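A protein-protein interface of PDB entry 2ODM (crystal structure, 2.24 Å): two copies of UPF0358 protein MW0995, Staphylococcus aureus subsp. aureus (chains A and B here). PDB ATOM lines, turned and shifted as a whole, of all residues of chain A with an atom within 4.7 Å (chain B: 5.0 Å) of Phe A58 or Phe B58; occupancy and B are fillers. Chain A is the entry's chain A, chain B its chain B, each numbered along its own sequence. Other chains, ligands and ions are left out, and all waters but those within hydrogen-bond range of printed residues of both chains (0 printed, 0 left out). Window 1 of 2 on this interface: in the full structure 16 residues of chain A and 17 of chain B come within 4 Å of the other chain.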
ATOM      1  N   ALA A  11      -0.141 -13.078  12.036  1.00  0.00           N
ATOM      2  CA  ALA A  11      -1.184 -12.246  12.631  1.00  0.00           C
ATOM      3  C   ALA A  11      -2.494 -13.012  12.721  1.00  0.00           C
ATOM      4  O   ALA A  11      -3.121 -13.063  13.786  1.00  0.00           O
ATOM      5  CB  ALA A  11      -1.360 -10.947  11.840  1.00  0.00           C
ATOM      6  N   GLN A  14      -2.198 -15.588  15.609  1.00  0.00           N
ATOM      7  CA  GLN A  14      -2.325 -15.042  16.963  1.00  0.00           C
ATOM      8  C   GLN A  14      -3.776 -14.674  17.290  1.00  0.00           C
ATOM      9  O   GLN A  14      -4.266 -14.947  18.385  1.00  0.00           O
ATOM     10  CB  GLN A  14      -1.399 -13.832  17.137  1.00  0.00           C
ATOM     11  CG  GLN A  14      -1.247 -13.335  18.578  1.00  0.00           C
ATOM     12  CD  GLN A  14      -0.835 -14.433  19.543  1.00  0.00           C
ATOM     13  OE1 GLN A  14      -1.538 -14.714  20.512  1.00  0.00           O
ATOM     14  NE2 GLN A  14       0.303 -15.067  19.274  1.00  0.00           N
ATOM     15  N   LEU A  15      -4.454 -14.081  16.312  1.00  0.00           N
ATOM     16  CA  LEU A  15      -5.827 -13.610  16.454  1.00  0.00           C
ATOM     17  C   LEU A  15      -6.796 -14.754  16.720  1.00  0.00           C
ATOM     18  O   LEU A  15      -7.691 -14.637  17.561  1.00  0.00           O
ATOM     19  CB  LEU A  15      -6.230 -12.862  15.180  1.00  0.00           C
ATOM     20  CG  LEU A  15      -6.999 -11.542  15.220  1.00  0.00           C
ATOM     21  CD1 LEU A  15      -6.409 -10.556  16.214  1.00  0.00           C
ATOM     22  CD2 LEU A  15      -7.002 -10.944  13.830  1.00  0.00           C
ATOM     23  N   ASP A  18      -6.227 -16.160  20.129  1.00  0.00           N
ATOM     24  CA  ASP A  18      -6.861 -15.276  21.095  1.00  0.00           C
ATOM     25  C   ASP A  18      -8.378 -15.450  21.129  1.00  0.00           C
ATOM     26  O   ASP A  18      -8.982 -15.431  22.204  1.00  0.00           O
ATOM     27  CB  ASP A  18      -6.454 -13.814  20.846  1.00  0.00           C
ATOM     28  CG  ASP A  18      -4.974 -13.569  21.120  1.00  0.00           C
ATOM     29  OD1 ASP A  18      -4.348 -14.405  21.807  1.00  0.00           O
ATOM     30  OD2 ASP A  18      -4.427 -12.548  20.653  1.00  0.00           O
ATOM     31  N   LYS A  54     -10.855  -5.052  19.173  1.00  0.00           N
ATOM     32  CA  LYS A  54      -9.775  -4.064  19.030  1.00  0.00           C
ATOM     33  C   LYS A  54      -8.494  -4.647  18.408  1.00  0.00           C
ATOM     34  O   LYS A  54      -7.830  -3.974  17.621  1.00  0.00           O
ATOM     35  CB  LYS A  54      -9.466  -3.374  20.371  1.00  0.00           C
ATOM     36  CG  LYS A  54     -10.617  -2.521  20.957  1.00  0.00           C
ATOM     37  CD  LYS A  54     -10.659  -1.091  20.412  1.00  0.00           C
ATOM     38  CE  LYS A  54     -11.661  -0.932  19.281  1.00  0.00           C
ATOM     39  NZ  LYS A  54     -13.070  -1.044  19.749  1.00  0.00           N
ATOM     40  N   GLU A  55      -8.142  -5.881  18.766  1.00  0.00           N
ATOM     41  CA  GLU A  55      -7.041  -6.597  18.103  1.00  0.00           C
ATOM     42  C   GLU A  55      -7.337  -6.797  16.613  1.00  0.00           C
ATOM     43  O   GLU A  55      -6.466  -6.604  15.762  1.00  0.00           O
ATOM     44  CB  GLU A  55      -6.832  -7.974  18.729  1.00  0.00           C
ATOM     45  CG  GLU A  55      -6.169  -8.012  20.088  1.00  0.00           C
ATOM     46  CD  GLU A  55      -6.004  -9.445  20.587  1.00  0.00           C
ATOM     47  OE1 GLU A  55      -5.524 -10.290  19.810  1.00  0.00           O
ATOM     48  OE2 GLU A  55      -6.362  -9.727  21.746  1.00  0.00           O
ATOM     49  N   VAL A  56      -8.570  -7.213  16.327  1.00  0.00           N
ATOM     50  CA  VAL A  56      -9.058  -7.438  14.966  1.00  0.00           C
ATOM     51  C   VAL A  56      -9.006  -6.151  14.140  1.00  0.00           C
ATOM     52  O   VAL A  56      -8.390  -6.132  13.072  1.00  0.00           O
ATOM     53  CB  VAL A  56     -10.495  -8.056  14.964  1.00  0.00           C
ATOM     54  CG1 VAL A  56     -11.146  -7.937  13.595  1.00  0.00           C
ATOM     55  CG2 VAL A  56     -10.441  -9.517  15.401  1.00  0.00           C
ATOM     56  N   ASP A  57      -9.632  -5.086  14.640  1.00  0.00           N
ATOM     57  CA  ASP A  57      -9.604  -3.780  13.955  1.00  0.00           C
ATOM     58  C   ASP A  57      -8.173  -3.319  13.705  1.00  0.00           C
ATOM     59  O   ASP A  57      -7.849  -2.862  12.608  1.00  0.00           O
ATOM     60  CB  ASP A  57     -10.354  -2.707  14.752  1.00  0.00           C
ATOM     61  CG  ASP A  57     -11.840  -2.984  14.871  1.00  0.00           C
ATOM     62  OD1 ASP A  57     -12.374  -3.788  14.076  1.00  0.00           O
ATOM     63  OD2 ASP A  57     -12.478  -2.386  15.767  1.00  0.00           O
ATOM     64  N   PHE A  58      -7.328  -3.446  14.729  1.00  0.00           N
ATOM     65  CA  PHE A  58      -5.906  -3.077  14.654  1.00  0.00           C
ATOM     66  C   PHE A  58      -5.186  -3.812  13.517  1.00  0.00           C
ATOM     67  O   PHE A  58      -4.411  -3.208  12.770  1.00  0.00           O
ATOM     68  CB  PHE A  58      -5.230  -3.362  16.005  1.00  0.00           C
ATOM     69  CG  PHE A  58      -3.744  -3.087  16.033  1.00  0.00           C
ATOM     70  CD1 PHE A  58      -3.259  -1.780  16.067  1.00  0.00           C
ATOM     71  CD2 PHE A  58      -2.832  -4.139  16.072  1.00  0.00           C
ATOM     72  CE1 PHE A  58      -1.883  -1.525  16.104  1.00  0.00           C
ATOM     73  CE2 PHE A  58      -1.454  -3.897  16.111  1.00  0.00           C
ATOM     74  CZ  PHE A  58      -0.980  -2.583  16.127  1.00  0.00           C
ATOM     75  N   ALA A  59      -5.454  -5.112  13.393  1.00  0.00           N
ATOM     76  CA  ALA A  59      -4.863  -5.951  12.344  1.00  0.00           C
ATOM     77  C   ALA A  59      -5.451  -5.650  10.968  1.00  0.00           C
ATOM     78  O   ALA A  59      -4.735  -5.655   9.963  1.00  0.00           O
ATOM     79  CB  ALA A  59      -5.028  -7.430  12.689  1.00  0.00           C
ATOM     80  N   VAL A  60      -6.755  -5.389  10.922  1.00  0.00           N
ATOM     81  CA  VAL A  60      -7.426  -5.035   9.673  1.00  0.00           C
ATOM     82  C   VAL A  60      -6.909  -3.698   9.122  1.00  0.00           C
ATOM     83  O   VAL A  60      -6.632  -3.588   7.924  1.00  0.00           O
ATOM     84  CB  VAL A  60      -8.973  -5.046   9.820  1.00  0.00           C
ATOM     85  CG1 VAL A  60      -9.642  -4.378   8.626  1.00  0.00           C
ATOM     86  CG2 VAL A  60      -9.482  -6.480   9.957  1.00  0.00           C
ATOM     87  N   LYS A  61      -6.755  -2.702   9.999  1.00  0.00           N
ATOM     88  CA  LYS A  61      -6.218  -1.393   9.617  1.00  0.00           C
ATOM     89  C   LYS A  61      -4.836  -1.486   8.971  1.00  0.00           C
ATOM     90  O   LYS A  61      -4.561  -0.813   7.977  1.00  0.00           O
ATOM     91  CB  LYS A  61      -6.146  -0.444  10.817  1.00  0.00           C
ATOM     92  CG  LYS A  61      -7.187   0.666  10.808  1.00  0.00           C
ATOM     93  CD  LYS A  61      -8.155   0.566  11.982  1.00  0.00           C
ATOM     94  CE  LYS A  61      -7.595   1.263  13.216  1.00  0.00           C
ATOM     95  NZ  LYS A  61      -8.656   1.588  14.206  1.00  0.00           N
ATOM     96  N   LEU A  62      -3.975  -2.323   9.542  1.00  0.00           N
ATOM     97  CA  LEU A  62      -2.601  -2.436   9.079  1.00  0.00           C
ATOM     98  C   LEU A  62      -2.480  -3.353   7.870  1.00  0.00           C
ATOM     99  O   LEU A  62      -1.378  -3.585   7.374  1.00  0.00           O
ATOM    100  CB  LEU A  62      -1.691  -2.936  10.203  1.00  0.00           C
ATOM    101  CG  LEU A  62      -1.444  -2.058  11.430  1.00  0.00           C
ATOM    102  CD1 LEU A  62      -0.658  -2.863  12.450  1.00  0.00           C
ATOM    103  CD2 LEU A  62      -0.707  -0.763  11.070  1.00  0.00           C
ATOM    104  N   LEU A  64      -2.773  -6.427   7.871  1.00  0.00           N
ATOM    105  CA  LEU A  64      -2.167  -7.682   8.320  1.00  0.00           C
ATOM    106  C   LEU A  64      -3.155  -8.820   8.157  1.00  0.00           C
ATOM    107  O   LEU A  64      -2.770  -9.969   7.964  1.00  0.00           O
ATOM    108  CB  LEU A  64      -1.762  -7.600   9.792  1.00  0.00           C
ATOM    109  CG  LEU A  64      -0.599  -6.717  10.236  1.00  0.00           C
ATOM    110  CD1 LEU A  64      -0.522  -6.722  11.750  1.00  0.00           C
ATOM    111  CD2 LEU A  64       0.715  -7.176   9.623  1.00  0.00           C
ATOM    112  N   ALA B  11       2.748   0.193  12.712  1.00  0.00           N
ATOM    113  CA  ALA B  11       2.144  -0.452  13.886  1.00  0.00           C
ATOM    114  C   ALA B  11       2.343   0.347  15.176  1.00  0.00           C
ATOM    115  O   ALA B  11       1.418   0.469  15.969  1.00  0.00           O
ATOM    116  CB  ALA B  11       2.686  -1.866  14.057  1.00  0.00           C
ATOM    117  N   GLN B  14      -0.005   3.385  14.630  1.00  0.00           N
ATOM    118  CA  GLN B  14      -1.415   3.049  14.850  1.00  0.00           C
ATOM    119  C   GLN B  14      -1.733   2.854  16.332  1.00  0.00           C
ATOM    120  O   GLN B  14      -2.817   3.196  16.789  1.00  0.00           O
ATOM    121  CB  GLN B  14      -1.796   1.794  14.056  1.00  0.00           C
ATOM    122  CG  GLN B  14      -3.281   1.424  14.117  1.00  0.00           C
ATOM    123  CD  GLN B  14      -4.186   2.539  13.620  1.00  0.00           C
ATOM    124  OE1 GLN B  14      -4.991   3.084  14.377  1.00  0.00           O
ATOM    125  NE2 GLN B  14      -4.046   2.896  12.346  1.00  0.00           N
ATOM    126  N   LEU B  15      -0.766   2.322  17.073  1.00  0.00           N
ATOM    127  CA  LEU B  15      -0.898   2.071  18.502  1.00  0.00           C
ATOM    128  C   LEU B  15      -0.882   3.366  19.319  1.00  0.00           C
ATOM    129  O   LEU B  15      -1.631   3.501  20.296  1.00  0.00           O
ATOM    130  CB  LEU B  15       0.244   1.161  18.949  1.00  0.00           C
ATOM    131  CG  LEU B  15       0.058  -0.034  19.882  1.00  0.00           C
ATOM    132  CD1 LEU B  15      -1.237  -0.804  19.625  1.00  0.00           C
ATOM    133  CD2 LEU B  15       1.269  -0.952  19.715  1.00  0.00           C
ATOM    134  N   ASP B  18      -4.168   5.210  18.607  1.00  0.00           N
ATOM    135  CA  ASP B  18      -5.201   4.629  19.477  1.00  0.00           C
ATOM    136  C   ASP B  18      -5.053   5.091  20.927  1.00  0.00           C
ATOM    137  O   ASP B  18      -6.031   5.452  21.570  1.00  0.00           O
ATOM    138  CB  ASP B  18      -5.185   3.093  19.396  1.00  0.00           C
ATOM    139  CG  ASP B  18      -5.550   2.573  18.006  1.00  0.00           C
ATOM    140  OD1 ASP B  18      -6.081   3.358  17.189  1.00  0.00           O
ATOM    141  OD2 ASP B  18      -5.297   1.382  17.718  1.00  0.00           O
ATOM    142  N   GLN B  53      -4.558  -2.306  25.739  1.00  0.00           N
ATOM    143  CA  GLN B  53      -3.634  -3.329  26.249  1.00  0.00           C
ATOM    144  C   GLN B  53      -3.613  -4.589  25.370  1.00  0.00           C
ATOM    145  O   GLN B  53      -2.550  -5.166  25.130  1.00  0.00           O
ATOM    146  CB  GLN B  53      -3.990  -3.695  27.696  1.00  0.00           C
ATOM    147  CG  GLN B  53      -2.976  -4.625  28.380  1.00  0.00           C
ATOM    148  CD  GLN B  53      -1.678  -3.921  28.738  1.00  0.00           C
ATOM    149  OE1 GLN B  53      -1.629  -3.134  29.680  1.00  0.00           O
ATOM    150  NE2 GLN B  53      -0.622  -4.204  27.987  1.00  0.00           N
ATOM    151  N   LYS B  54      -4.784  -4.996  24.883  1.00  0.00           N
ATOM    152  CA  LYS B  54      -4.900  -6.154  23.981  1.00  0.00           C
ATOM    153  C   LYS B  54      -4.186  -5.946  22.654  1.00  0.00           C
ATOM    154  O   LYS B  54      -3.504  -6.850  22.172  1.00  0.00           O
ATOM    155  CB  LYS B  54      -6.369  -6.543  23.750  1.00  0.00           C
ATOM    156  CG  LYS B  54      -7.066  -7.087  25.000  1.00  0.00           C
ATOM    157  CD  LYS B  54      -6.232  -8.180  25.663  1.00  0.00           C
ATOM    158  CE  LYS B  54      -6.107  -7.928  27.160  1.00  0.00           C
ATOM    159  NZ  LYS B  54      -4.915  -8.600  27.762  1.00  0.00           N
ATOM    160  N   GLU B  55      -4.339  -4.754  22.073  1.00  0.00           N
ATOM    161  CA  GLU B  55      -3.621  -4.384  20.852  1.00  0.00           C
ATOM    162  C   GLU B  55      -2.115  -4.364  21.081  1.00  0.00           C
ATOM    163  O   GLU B  55      -1.349  -4.814  20.233  1.00  0.00           O
ATOM    164  CB  GLU B  55      -4.039  -2.998  20.358  1.00  0.00           C
ATOM    165  CG  GLU B  55      -5.496  -2.811  20.016  1.00  0.00           C
ATOM    166  CD  GLU B  55      -5.791  -1.394  19.527  1.00  0.00           C
ATOM    167  OE1 GLU B  55      -4.866  -0.550  19.529  1.00  0.00           O
ATOM    168  OE2 GLU B  55      -6.945  -1.127  19.127  1.00  0.00           O
ATOM    169  N   VAL B  56      -1.696  -3.802  22.212  1.00  0.00           N
ATOM    170  CA  VAL B  56      -0.276  -3.700  22.544  1.00  0.00           C
ATOM    171  C   VAL B  56       0.377  -5.082  22.610  1.00  0.00           C
ATOM    172  O   VAL B  56       1.345  -5.331  21.891  1.00  0.00           O
ATOM    173  CB  VAL B  56      -0.034  -2.896  23.859  1.00  0.00           C
ATOM    174  CG1 VAL B  56       1.373  -3.126  24.380  1.00  0.00           C
ATOM    175  CG2 VAL B  56      -0.258  -1.400  23.622  1.00  0.00           C
ATOM    176  N   ASP B  57      -0.162  -5.969  23.455  1.00  0.00           N
ATOM    177  CA  ASP B  57       0.331  -7.356  23.585  1.00  0.00           C
ATOM    178  C   ASP B  57       0.369  -8.076  22.243  1.00  0.00           C
ATOM    179  O   ASP B  57       1.362  -8.712  21.907  1.00  0.00           O
ATOM    180  CB  ASP B  57      -0.531  -8.168  24.558  1.00  0.00           C
ATOM    181  CG  ASP B  57      -0.629  -7.535  25.921  1.00  0.00           C
ATOM    182  OD1 ASP B  57       0.234  -6.697  26.267  1.00  0.00           O
ATOM    183  OD2 ASP B  57      -1.587  -7.871  26.652  1.00  0.00           O
ATOM    184  N   PHE B  58      -0.725  -7.965  21.491  1.00  0.00           N
ATOM    185  CA  PHE B  58      -0.824  -8.513  20.143  1.00  0.00           C
ATOM    186  C   PHE B  58       0.362  -8.085  19.272  1.00  0.00           C
ATOM    187  O   PHE B  58       1.040  -8.933  18.692  1.00  0.00           O
ATOM    188  CB  PHE B  58      -2.169  -8.110  19.508  1.00  0.00           C
ATOM    189  CG  PHE B  58      -2.376  -8.630  18.110  1.00  0.00           C
ATOM    190  CD1 PHE B  58      -2.265  -7.778  17.015  1.00  0.00           C
ATOM    191  CD2 PHE B  58      -2.687  -9.967  17.888  1.00  0.00           C
ATOM    192  CE1 PHE B  58      -2.451  -8.249  15.726  1.00  0.00           C
ATOM    193  CE2 PHE B  58      -2.872 -10.453  16.596  1.00  0.00           C
ATOM    194  CZ  PHE B  58      -2.760  -9.592  15.514  1.00  0.00           C
ATOM    195  N   ALA B  59       0.625  -6.778  19.207  1.00  0.00           N
ATOM    196  CA  ALA B  59       1.748  -6.245  18.425  1.00  0.00           C
ATOM    197  C   ALA B  59       3.124  -6.644  18.970  1.00  0.00           C
ATOM    198  O   ALA B  59       4.064  -6.846  18.200  1.00  0.00           O
ATOM    199  CB  ALA B  59       1.643  -4.724  18.298  1.00  0.00           C
ATOM    200  N   VAL B  60       3.240  -6.745  20.291  1.00  0.00           N
ATOM    201  CA  VAL B  60       4.501  -7.122  20.935  1.00  0.00           C
ATOM    202  C   VAL B  60       4.831  -8.590  20.644  1.00  0.00           C
ATOM    203  O   VAL B  60       5.968  -8.917  20.286  1.00  0.00           O
ATOM    204  CB  VAL B  60       4.482  -6.837  22.468  1.00  0.00           C
ATOM    205  CG1 VAL B  60       5.713  -7.427  23.163  1.00  0.00           C
ATOM    206  CG2 VAL B  60       4.394  -5.336  22.737  1.00  0.00           C
ATOM    207  N   LYS B  61       3.824  -9.455  20.777  1.00  0.00           N
ATOM    208  CA  LYS B  61       3.946 -10.881  20.454  1.00  0.00           C
ATOM    209  C   LYS B  61       4.392 -11.136  19.012  1.00  0.00           C
ATOM    210  O   LYS B  61       5.168 -12.055  18.748  1.00  0.00           O
ATOM    211  CB  LYS B  61       2.624 -11.612  20.717  1.00  0.00           C
ATOM    212  CG  LYS B  61       2.302 -11.817  22.188  1.00  0.00           C
ATOM    213  CD  LYS B  61       0.951 -12.495  22.361  1.00  0.00           C
ATOM    214  CE  LYS B  61       0.509 -12.467  23.809  1.00  0.00           C
ATOM    215  NZ  LYS B  61      -0.888 -12.956  23.969  1.00  0.00           N
ATOM    216  N   LEU B  62       3.901 -10.323  18.084  1.00  0.00           N
ATOM    217  CA  LEU B  62       4.225 -10.492  16.672  1.00  0.00           C
ATOM    218  C   LEU B  62       5.566  -9.865  16.277  1.00  0.00           C
ATOM    219  O   LEU B  62       5.995  -9.983  15.127  1.00  0.00           O
ATOM    220  CB  LEU B  62       3.096  -9.952  15.794  1.00  0.00           C
ATOM    221  CG  LEU B  62       1.721 -10.617  15.901  1.00  0.00           C
ATOM    222  CD1 LEU B  62       0.716  -9.814  15.101  1.00  0.00           C
ATOM    223  CD2 LEU B  62       1.749 -12.062  15.428  1.00  0.00           C
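Of the 14 printed residues of chain B, 9 touch a printed residue of chain A. Of the 14 printed residues of chain A, 8 touch a printed residue of chain B. Among the printed residues, 16 pairs touch across the chains. Among the printed residues, no Asp or Glu carboxylate lies within 4 Å of a Lys or Arg side-chain nitrogen of the other chain.
The backbone carbonyl oxygen (O) of Lys A54 lies close to the side-chain carboxylate (OE2) of Glu B55 (3.3 Å).
The side-chain amide oxygen of Gln A14 lies close to the side-chain carboxylate of Asp A18, at 3.1 Å. The side-chain carboxylate of Asp A18 sits close to the side-chain carboxylate of Glu A55 (2.6 Å). The side-chain amide oxygen of Gln B14 sits close to the side-chain carboxylate of Asp B18, at 3.0 Å. The side-chain carboxylate (OD2) of Asp B18 sits close to the side-chain carboxylate (OE1) of Glu B55, 2.7 Å away. The side-chain amino group (NZ) of Lys B54 is in salt-bridge range of the side-chain carboxylate (OD2) of Asp B57, 3.6 Å away.
Among the printed residues, pairs that only touch across the chains: Ala A11 with Phe B58, Ala A11 with Leu B62, Gln A14 with Phe B58, Gln A14 with Lys B61, Gln A14 with Leu B62, Leu A15 with Phe B58, Glu A55 with Lys B54, Glu A55 with Phe B58, Phe A58 with Ala B11, Phe A58 with Gln B14, Phe A58 with Leu B15, Phe A58 with Phe B58, Phe A58 with Ala B59, Lys A61 with Gln B14 and Leu A62 with Ala B11.
Ala A11 touches Phe B58, and with the chains exchanged Phe A58 touches Ala B11. Gln A14 touches Lys B61, and with the chains exchanged Lys A61 touches Gln B14. Glu A55 touches Phe B58, but with the chains exchanged Phe A58 does not touch Glu B55 (4.01 Å). Phe A58 touches Ala B59, but with the chains exchanged Ala A59 does not touch Phe B58 (4.1 Å). Of the 16 pairs that touch across the chains among the printed residues, 13 have their exchanged pair printed and touching as well.
Of the printed residues of chain B, Phe A58 touches Ala B11 (3.9 Å), Gln B14 (3.8 Å), Leu B15 (3.7 Å), Phe B58 (3.8 Å) and Ala B59 (3.9 Å). Of chain A, only Ala A11 (3.8 Å), Gln A14 (3.7 Å), Leu A15 (3.6 Å), Glu A55 (3.4 Å) and Phe A58 (3.8 Å) come within 4 Å of Phe B58. Of the printed residues of chain B, Leu A62 touches Ala B11. Printed residues of chain A within 4 Å of Leu B15: Phe A58 (3.7 Å). Val A60 touches none of the printed residues of chain B. Leu A64 touches none of the printed residues of chain B. The nearest printed residue of chain B that does not touch Phe A58 is Glu B55 (4.01 Å). The nearest residue of chain A that does not touch Phe B58 is Ala A59 (4.1 Å). The nearest printed residue of chain B that does not touch Leu A15 is Leu B62 (6.6 Å).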
